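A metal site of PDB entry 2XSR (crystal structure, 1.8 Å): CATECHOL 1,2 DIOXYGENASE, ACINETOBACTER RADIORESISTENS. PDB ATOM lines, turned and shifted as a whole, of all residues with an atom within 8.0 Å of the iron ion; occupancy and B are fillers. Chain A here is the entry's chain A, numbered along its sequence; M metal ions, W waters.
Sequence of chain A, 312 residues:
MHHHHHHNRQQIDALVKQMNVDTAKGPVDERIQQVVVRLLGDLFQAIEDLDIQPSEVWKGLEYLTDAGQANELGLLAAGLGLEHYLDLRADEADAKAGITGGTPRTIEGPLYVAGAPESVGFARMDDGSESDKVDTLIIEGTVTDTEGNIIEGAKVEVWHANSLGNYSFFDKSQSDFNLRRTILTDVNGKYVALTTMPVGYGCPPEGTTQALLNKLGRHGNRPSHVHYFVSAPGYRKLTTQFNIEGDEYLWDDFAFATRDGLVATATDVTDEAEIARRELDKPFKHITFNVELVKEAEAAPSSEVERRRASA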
ATOM      1  N   ILE A 107     -21.222   2.709 -27.425  1.00  0.00           N
ATOM      2  CA  ILE A 107     -21.766   2.598 -26.060  1.00  0.00           C
ATOM      3  C   ILE A 107     -22.851   3.638 -25.772  1.00  0.00           C
ATOM      4  O   ILE A 107     -22.829   4.766 -26.321  1.00  0.00           O
ATOM      5  CB  ILE A 107     -20.661   2.644 -24.948  1.00  0.00           C
ATOM      6  CG1 ILE A 107     -20.135   4.081 -24.748  1.00  0.00           C
ATOM      7  CG2 ILE A 107     -19.544   1.604 -25.292  1.00  0.00           C
ATOM      8  CD1 ILE A 107     -19.029   4.256 -23.652  1.00  0.00           C
ATOM      9  N   GLU A 108     -23.801   3.236 -24.942  1.00  0.00           N
ATOM     10  CA  GLU A 108     -24.883   4.129 -24.480  1.00  0.00           C
ATOM     11  C   GLU A 108     -24.355   5.223 -23.528  1.00  0.00           C
ATOM     12  O   GLU A 108     -24.808   6.361 -23.547  1.00  0.00           O
ATOM     13  CB  GLU A 108     -25.929   3.274 -23.747  1.00  0.00           C
ATOM     14  CG  GLU A 108     -27.204   4.038 -23.292  1.00  0.00           C
ATOM     15  CD  GLU A 108     -28.213   3.107 -22.618  1.00  0.00           C
ATOM     16  OE1 GLU A 108     -28.351   1.950 -23.085  1.00  0.00           O
ATOM     17  OE2 GLU A 108     -28.881   3.542 -21.625  1.00  0.00           O
ATOM     18  N   GLY A 109     -23.401   4.828 -22.677  1.00  0.00           N
ATOM     19  CA  GLY A 109     -22.987   5.623 -21.492  1.00  0.00           C
ATOM     20  C   GLY A 109     -24.095   5.616 -20.441  1.00  0.00           C
ATOM     21  O   GLY A 109     -25.178   5.052 -20.675  1.00  0.00           O
ATOM     22  N   PRO A 110     -23.845   6.258 -19.280  1.00  0.00           N
ATOM     23  CA  PRO A 110     -24.724   6.144 -18.133  1.00  0.00           C
ATOM     24  C   PRO A 110     -25.711   7.302 -17.962  1.00  0.00           C
ATOM     25  O   PRO A 110     -26.326   7.411 -16.891  1.00  0.00           O
ATOM     26  CB  PRO A 110     -23.715   6.142 -16.959  1.00  0.00           C
ATOM     27  CG  PRO A 110     -22.676   7.034 -17.402  1.00  0.00           C
ATOM     28  CD  PRO A 110     -22.528   6.799 -18.904  1.00  0.00           C
ATOM     29  N   LEU A 111     -25.920   8.115 -19.004  1.00  0.00           N
ATOM     30  CA  LEU A 111     -26.630   9.410 -18.809  1.00  0.00           C
ATOM     31  C   LEU A 111     -27.917   9.600 -19.631  1.00  0.00           C
ATOM     32  O   LEU A 111     -28.451  10.735 -19.722  1.00  0.00           O
ATOM     33  CB  LEU A 111     -25.674  10.597 -19.022  1.00  0.00           C
ATOM     34  CG  LEU A 111     -24.370  10.600 -18.213  1.00  0.00           C
ATOM     35  CD1 LEU A 111     -23.512  11.770 -18.639  1.00  0.00           C
ATOM     36  CD2 LEU A 111     -24.606  10.590 -16.668  1.00  0.00           C
ATOM     37  N   TYR A 112     -28.483   8.505 -20.141  1.00  0.00           N
ATOM     38  CA  TYR A 112     -29.777   8.596 -20.792  1.00  0.00           C
ATOM     39  C   TYR A 112     -30.876   8.875 -19.765  1.00  0.00           C
ATOM     40  O   TYR A 112     -30.786   8.370 -18.631  1.00  0.00           O
ATOM     41  CB  TYR A 112     -30.105   7.315 -21.541  1.00  0.00           C
ATOM     42  CG  TYR A 112     -31.501   7.298 -22.146  1.00  0.00           C
ATOM     43  CD1 TYR A 112     -31.787   8.007 -23.338  1.00  0.00           C
ATOM     44  CD2 TYR A 112     -32.530   6.568 -21.546  1.00  0.00           C
ATOM     45  CE1 TYR A 112     -33.082   7.979 -23.893  1.00  0.00           C
ATOM     46  CE2 TYR A 112     -33.819   6.534 -22.084  1.00  0.00           C
ATOM     47  CZ  TYR A 112     -34.090   7.227 -23.252  1.00  0.00           C
ATOM     48  OH  TYR A 112     -35.379   7.126 -23.788  1.00  0.00           O
ATOM     49  N   TRP A 159     -29.333  12.911 -27.141  1.00  0.00           N
ATOM     50  CA  TRP A 159     -28.995  13.661 -25.921  1.00  0.00           C
ATOM     51  C   TRP A 159     -27.519  14.027 -25.973  1.00  0.00           C
ATOM     52  O   TRP A 159     -26.707  13.295 -26.535  1.00  0.00           O
ATOM     53  CB  TRP A 159     -29.397  12.899 -24.621  1.00  0.00           C
ATOM     54  CG  TRP A 159     -28.667  11.552 -24.309  1.00  0.00           C
ATOM     55  CD1 TRP A 159     -27.709  11.350 -23.368  1.00  0.00           C
ATOM     56  CD2 TRP A 159     -28.918  10.258 -24.912  1.00  0.00           C
ATOM     57  NE1 TRP A 159     -27.330   9.995 -23.335  1.00  0.00           N
ATOM     58  CE2 TRP A 159     -28.062   9.326 -24.273  1.00  0.00           C
ATOM     59  CE3 TRP A 159     -29.774   9.811 -25.926  1.00  0.00           C
ATOM     60  CZ2 TRP A 159     -28.013   7.950 -24.641  1.00  0.00           C
ATOM     61  CZ3 TRP A 159     -29.749   8.433 -26.297  1.00  0.00           C
ATOM     62  CH2 TRP A 159     -28.854   7.519 -25.643  1.00  0.00           C
ATOM     63  N   HIS A 160     -27.165  15.194 -25.423  1.00  0.00           N
ATOM     64  CA  HIS A 160     -25.757  15.655 -25.444  1.00  0.00           C
ATOM     65  C   HIS A 160     -25.489  16.726 -24.387  1.00  0.00           C
ATOM     66  O   HIS A 160     -26.447  17.227 -23.759  1.00  0.00           O
ATOM     67  CB  HIS A 160     -25.321  16.135 -26.866  1.00  0.00           C
ATOM     68  CG  HIS A 160     -25.929  17.432 -27.323  1.00  0.00           C
ATOM     69  ND1 HIS A 160     -25.497  18.665 -26.867  1.00  0.00           N
ATOM     70  CD2 HIS A 160     -26.892  17.693 -28.256  1.00  0.00           C
ATOM     71  CE1 HIS A 160     -26.191  19.620 -27.467  1.00  0.00           C
ATOM     72  NE2 HIS A 160     -27.027  19.067 -28.333  1.00  0.00           N
ATOM     73  N   ALA A 161     -24.202  17.061 -24.207  1.00  0.00           N
ATOM     74  CA  ALA A 161     -23.756  17.990 -23.178  1.00  0.00           C
ATOM     75  C   ALA A 161     -23.868  19.450 -23.601  1.00  0.00           C
ATOM     76  O   ALA A 161     -23.883  19.778 -24.805  1.00  0.00           O
ATOM     77  CB  ALA A 161     -22.312  17.690 -22.809  1.00  0.00           C
ATOM     78  N   GLY A 165     -19.788  20.995 -20.929  1.00  0.00           N
ATOM     79  CA  GLY A 165     -19.647  19.529 -20.849  1.00  0.00           C
ATOM     80  C   GLY A 165     -20.580  18.846 -19.848  1.00  0.00           C
ATOM     81  O   GLY A 165     -20.303  17.717 -19.434  1.00  0.00           O
ATOM     82  N   TYR A 167     -24.554  17.531 -18.528  1.00  0.00           N
ATOM     83  CA  TYR A 167     -25.845  17.038 -19.031  1.00  0.00           C
ATOM     84  C   TYR A 167     -26.995  17.438 -18.093  1.00  0.00           C
ATOM     85  O   TYR A 167     -26.847  17.439 -16.865  1.00  0.00           O
ATOM     86  CB  TYR A 167     -25.838  15.500 -19.060  1.00  0.00           C
ATOM     87  CG  TYR A 167     -25.011  14.899 -20.182  1.00  0.00           C
ATOM     88  CD1 TYR A 167     -25.641  14.371 -21.298  1.00  0.00           C
ATOM     89  CD2 TYR A 167     -23.597  14.864 -20.116  1.00  0.00           C
ATOM     90  CE1 TYR A 167     -24.902  13.812 -22.365  1.00  0.00           C
ATOM     91  CE2 TYR A 167     -22.852  14.284 -21.159  1.00  0.00           C
ATOM     92  CZ  TYR A 167     -23.508  13.742 -22.259  1.00  0.00           C
ATOM     93  OH  TYR A 167     -22.799  13.180 -23.284  1.00  0.00           O
ATOM     94  N   VAL A 199     -19.423  20.091 -26.019  1.00  0.00           N
ATOM     95  CA  VAL A 199     -17.985  19.973 -25.723  1.00  0.00           C
ATOM     96  C   VAL A 199     -17.757  18.638 -24.993  1.00  0.00           C
ATOM     97  O   VAL A 199     -18.677  18.148 -24.378  1.00  0.00           O
ATOM     98  CB  VAL A 199     -17.483  21.215 -24.903  1.00  0.00           C
ATOM     99  CG1 VAL A 199     -18.019  21.213 -23.530  1.00  0.00           C
ATOM    100  CG2 VAL A 199     -16.018  21.256 -24.887  1.00  0.00           C
ATOM    101  N   TYR A 201     -15.756  16.303 -22.032  1.00  0.00           N
ATOM    102  CA  TYR A 201     -15.808  16.534 -20.597  1.00  0.00           C
ATOM    103  C   TYR A 201     -15.092  15.390 -19.943  1.00  0.00           C
ATOM    104  O   TYR A 201     -14.890  14.325 -20.564  1.00  0.00           O
ATOM    105  CB  TYR A 201     -17.268  16.526 -20.131  1.00  0.00           C
ATOM    106  CG  TYR A 201     -18.080  15.340 -20.640  1.00  0.00           C
ATOM    107  CD1 TYR A 201     -18.198  14.156 -19.866  1.00  0.00           C
ATOM    108  CD2 TYR A 201     -18.766  15.393 -21.843  1.00  0.00           C
ATOM    109  CE1 TYR A 201     -18.934  13.080 -20.311  1.00  0.00           C
ATOM    110  CE2 TYR A 201     -19.530  14.302 -22.295  1.00  0.00           C
ATOM    111  CZ  TYR A 201     -19.595  13.146 -21.530  1.00  0.00           C
ATOM    112  OH  TYR A 201     -20.331  12.071 -21.975  1.00  0.00           O
ATOM    113  N   ARG A 222     -13.734  12.405 -22.319  1.00  0.00           N
ATOM    114  CA  ARG A 222     -14.355  11.944 -23.571  1.00  0.00           C
ATOM    115  C   ARG A 222     -14.326  13.095 -24.590  1.00  0.00           C
ATOM    116  O   ARG A 222     -14.492  14.277 -24.209  1.00  0.00           O
ATOM    117  CB  ARG A 222     -15.852  11.593 -23.376  1.00  0.00           C
ATOM    118  CG  ARG A 222     -16.103  10.623 -22.236  1.00  0.00           C
ATOM    119  CD  ARG A 222     -17.394   9.859 -22.416  1.00  0.00           C
ATOM    120  NE  ARG A 222     -17.294   8.938 -23.552  1.00  0.00           N
ATOM    121  CZ  ARG A 222     -18.328   8.338 -24.144  1.00  0.00           C
ATOM    122  NH1 ARG A 222     -19.577   8.549 -23.693  1.00  0.00           N
ATOM    123  NH2 ARG A 222     -18.105   7.537 -25.175  1.00  0.00           N
ATOM    124  N   PRO A 223     -14.169  12.759 -25.895  1.00  0.00           N
ATOM    125  CA  PRO A 223     -14.333  13.779 -26.943  1.00  0.00           C
ATOM    126  C   PRO A 223     -15.799  14.175 -27.077  1.00  0.00           C
ATOM    127  O   PRO A 223     -16.701  13.421 -26.615  1.00  0.00           O
ATOM    128  CB  PRO A 223     -13.858  13.073 -28.218  1.00  0.00           C
ATOM    129  CG  PRO A 223     -14.215  11.576 -27.977  1.00  0.00           C
ATOM    130  CD  PRO A 223     -13.939  11.415 -26.458  1.00  0.00           C
ATOM    131  N   SER A 224     -16.042  15.330 -27.692  1.00  0.00           N
ATOM    132  CA  SER A 224     -17.408  15.788 -27.984  1.00  0.00           C
ATOM    133  C   SER A 224     -18.176  14.733 -28.798  1.00  0.00           C
ATOM    134  O   SER A 224     -17.606  14.087 -29.723  1.00  0.00           O
ATOM    135  CB  SER A 224     -17.379  17.090 -28.768  1.00  0.00           C
ATOM    136  OG  SER A 224     -16.656  16.883 -29.985  1.00  0.00           O
ATOM    137  N   HIS A 225     -19.458  14.567 -28.475  1.00  0.00           N
ATOM    138  CA  HIS A 225     -20.289  13.581 -29.180  1.00  0.00           C
ATOM    139  C   HIS A 225     -21.780  13.880 -28.949  1.00  0.00           C
ATOM    140  O   HIS A 225     -22.110  14.638 -28.049  1.00  0.00           O
ATOM    141  CB  HIS A 225     -19.978  12.153 -28.662  1.00  0.00           C
ATOM    142  CG  HIS A 225     -20.180  12.004 -27.184  1.00  0.00           C
ATOM    143  ND1 HIS A 225     -19.243  12.412 -26.266  1.00  0.00           N
ATOM    144  CD2 HIS A 225     -21.215  11.499 -26.468  1.00  0.00           C
ATOM    145  CE1 HIS A 225     -19.694  12.175 -25.038  1.00  0.00           C
ATOM    146  NE2 HIS A 225     -20.873  11.590 -25.135  1.00  0.00           N
ATOM    147  N   VAL A 226     -22.635  13.308 -29.781  1.00  0.00           N
ATOM    148  CA  VAL A 226     -24.078  13.356 -29.568  1.00  0.00           C
ATOM    149  C   VAL A 226     -24.575  11.910 -29.572  1.00  0.00           C
ATOM    150  O   VAL A 226     -24.268  11.144 -30.511  1.00  0.00           O
ATOM    151  CB  VAL A 226     -24.819  14.202 -30.659  1.00  0.00           C
ATOM    152  CG1 VAL A 226     -26.354  14.136 -30.473  1.00  0.00           C
ATOM    153  CG2 VAL A 226     -24.321  15.683 -30.646  1.00  0.00           C
ATOM    154  N   HIS A 227     -25.319  11.533 -28.530  1.00  0.00           N
ATOM    155  CA  HIS A 227     -25.814  10.152 -28.404  1.00  0.00           C
ATOM    156  C   HIS A 227     -27.107   9.968 -29.207  1.00  0.00           C
ATOM    157  O   HIS A 227     -27.931  10.890 -29.276  1.00  0.00           O
ATOM    158  CB  HIS A 227     -26.192   9.886 -26.935  1.00  0.00           C
ATOM    159  CG  HIS A 227     -25.049   9.841 -25.975  1.00  0.00           C
ATOM    160  ND1 HIS A 227     -24.328   8.698 -25.729  1.00  0.00           N
ATOM    161  CD2 HIS A 227     -24.530  10.809 -25.168  1.00  0.00           C
ATOM    162  CE1 HIS A 227     -23.392   8.954 -24.825  1.00  0.00           C
ATOM    163  NE2 HIS A 227     -23.497  10.221 -24.450  1.00  0.00           N
ATOM    164  N   GLN A 241     -23.594   6.912 -31.640  1.00  0.00           N
ATOM    165  CA  GLN A 241     -23.344   8.375 -31.491  1.00  0.00           C
ATOM    166  C   GLN A 241     -22.681   8.876 -32.764  1.00  0.00           C
ATOM    167  O   GLN A 241     -22.260   8.072 -33.611  1.00  0.00           O
ATOM    168  CB  GLN A 241     -22.416   8.666 -30.320  1.00  0.00           C
ATOM    169  CG  GLN A 241     -20.968   8.239 -30.542  1.00  0.00           C
ATOM    170  CD  GLN A 241     -20.114   8.260 -29.264  1.00  0.00           C
ATOM    171  OE1 GLN A 241     -20.638   8.322 -28.139  1.00  0.00           O
ATOM    172  NE2 GLN A 241     -18.809   8.216 -29.439  1.00  0.00           N
HETATM  173 FE    FE M   1     -22.144  11.338 -23.476  1.00  0.00          FE
HETATM  174  O   HOH W   1     -21.876   9.812 -21.640  1.00  0.00           O
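Arg 222 touches the iron ion.
Of the 20 residues printed, 5 come within 4 Å of the iron ion.
N of His 227 sits at hydrogen-bond distance from O of Trp 159 (3.0 Å).
The backbone carbonyl oxygen (O) of Glu 108 sits close to a ring nitrogen (ND1) of His 227 (3.2 Å).
ND1 of His 225 is in hydrogen-bond range of O of Pro 223, at 2.8 Å.
O of Tyr 201 lies within hydrogen-bond range of N of Arg 222 (2.8 Å).
OH of Tyr 167 is bound to the iron ion, 2.0 Å away.
NE2 of His 227 binds the iron ion (2.0 Å).
The iron ion is bound by a ring nitrogen (NE2) of His 225 (2.1 Å).
Water W1 is bound to the iron ion, at 2.4 Å.
The iron ion is bound by the side-chain hydroxyl (OH) of Tyr 201, 2.5 Å away.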
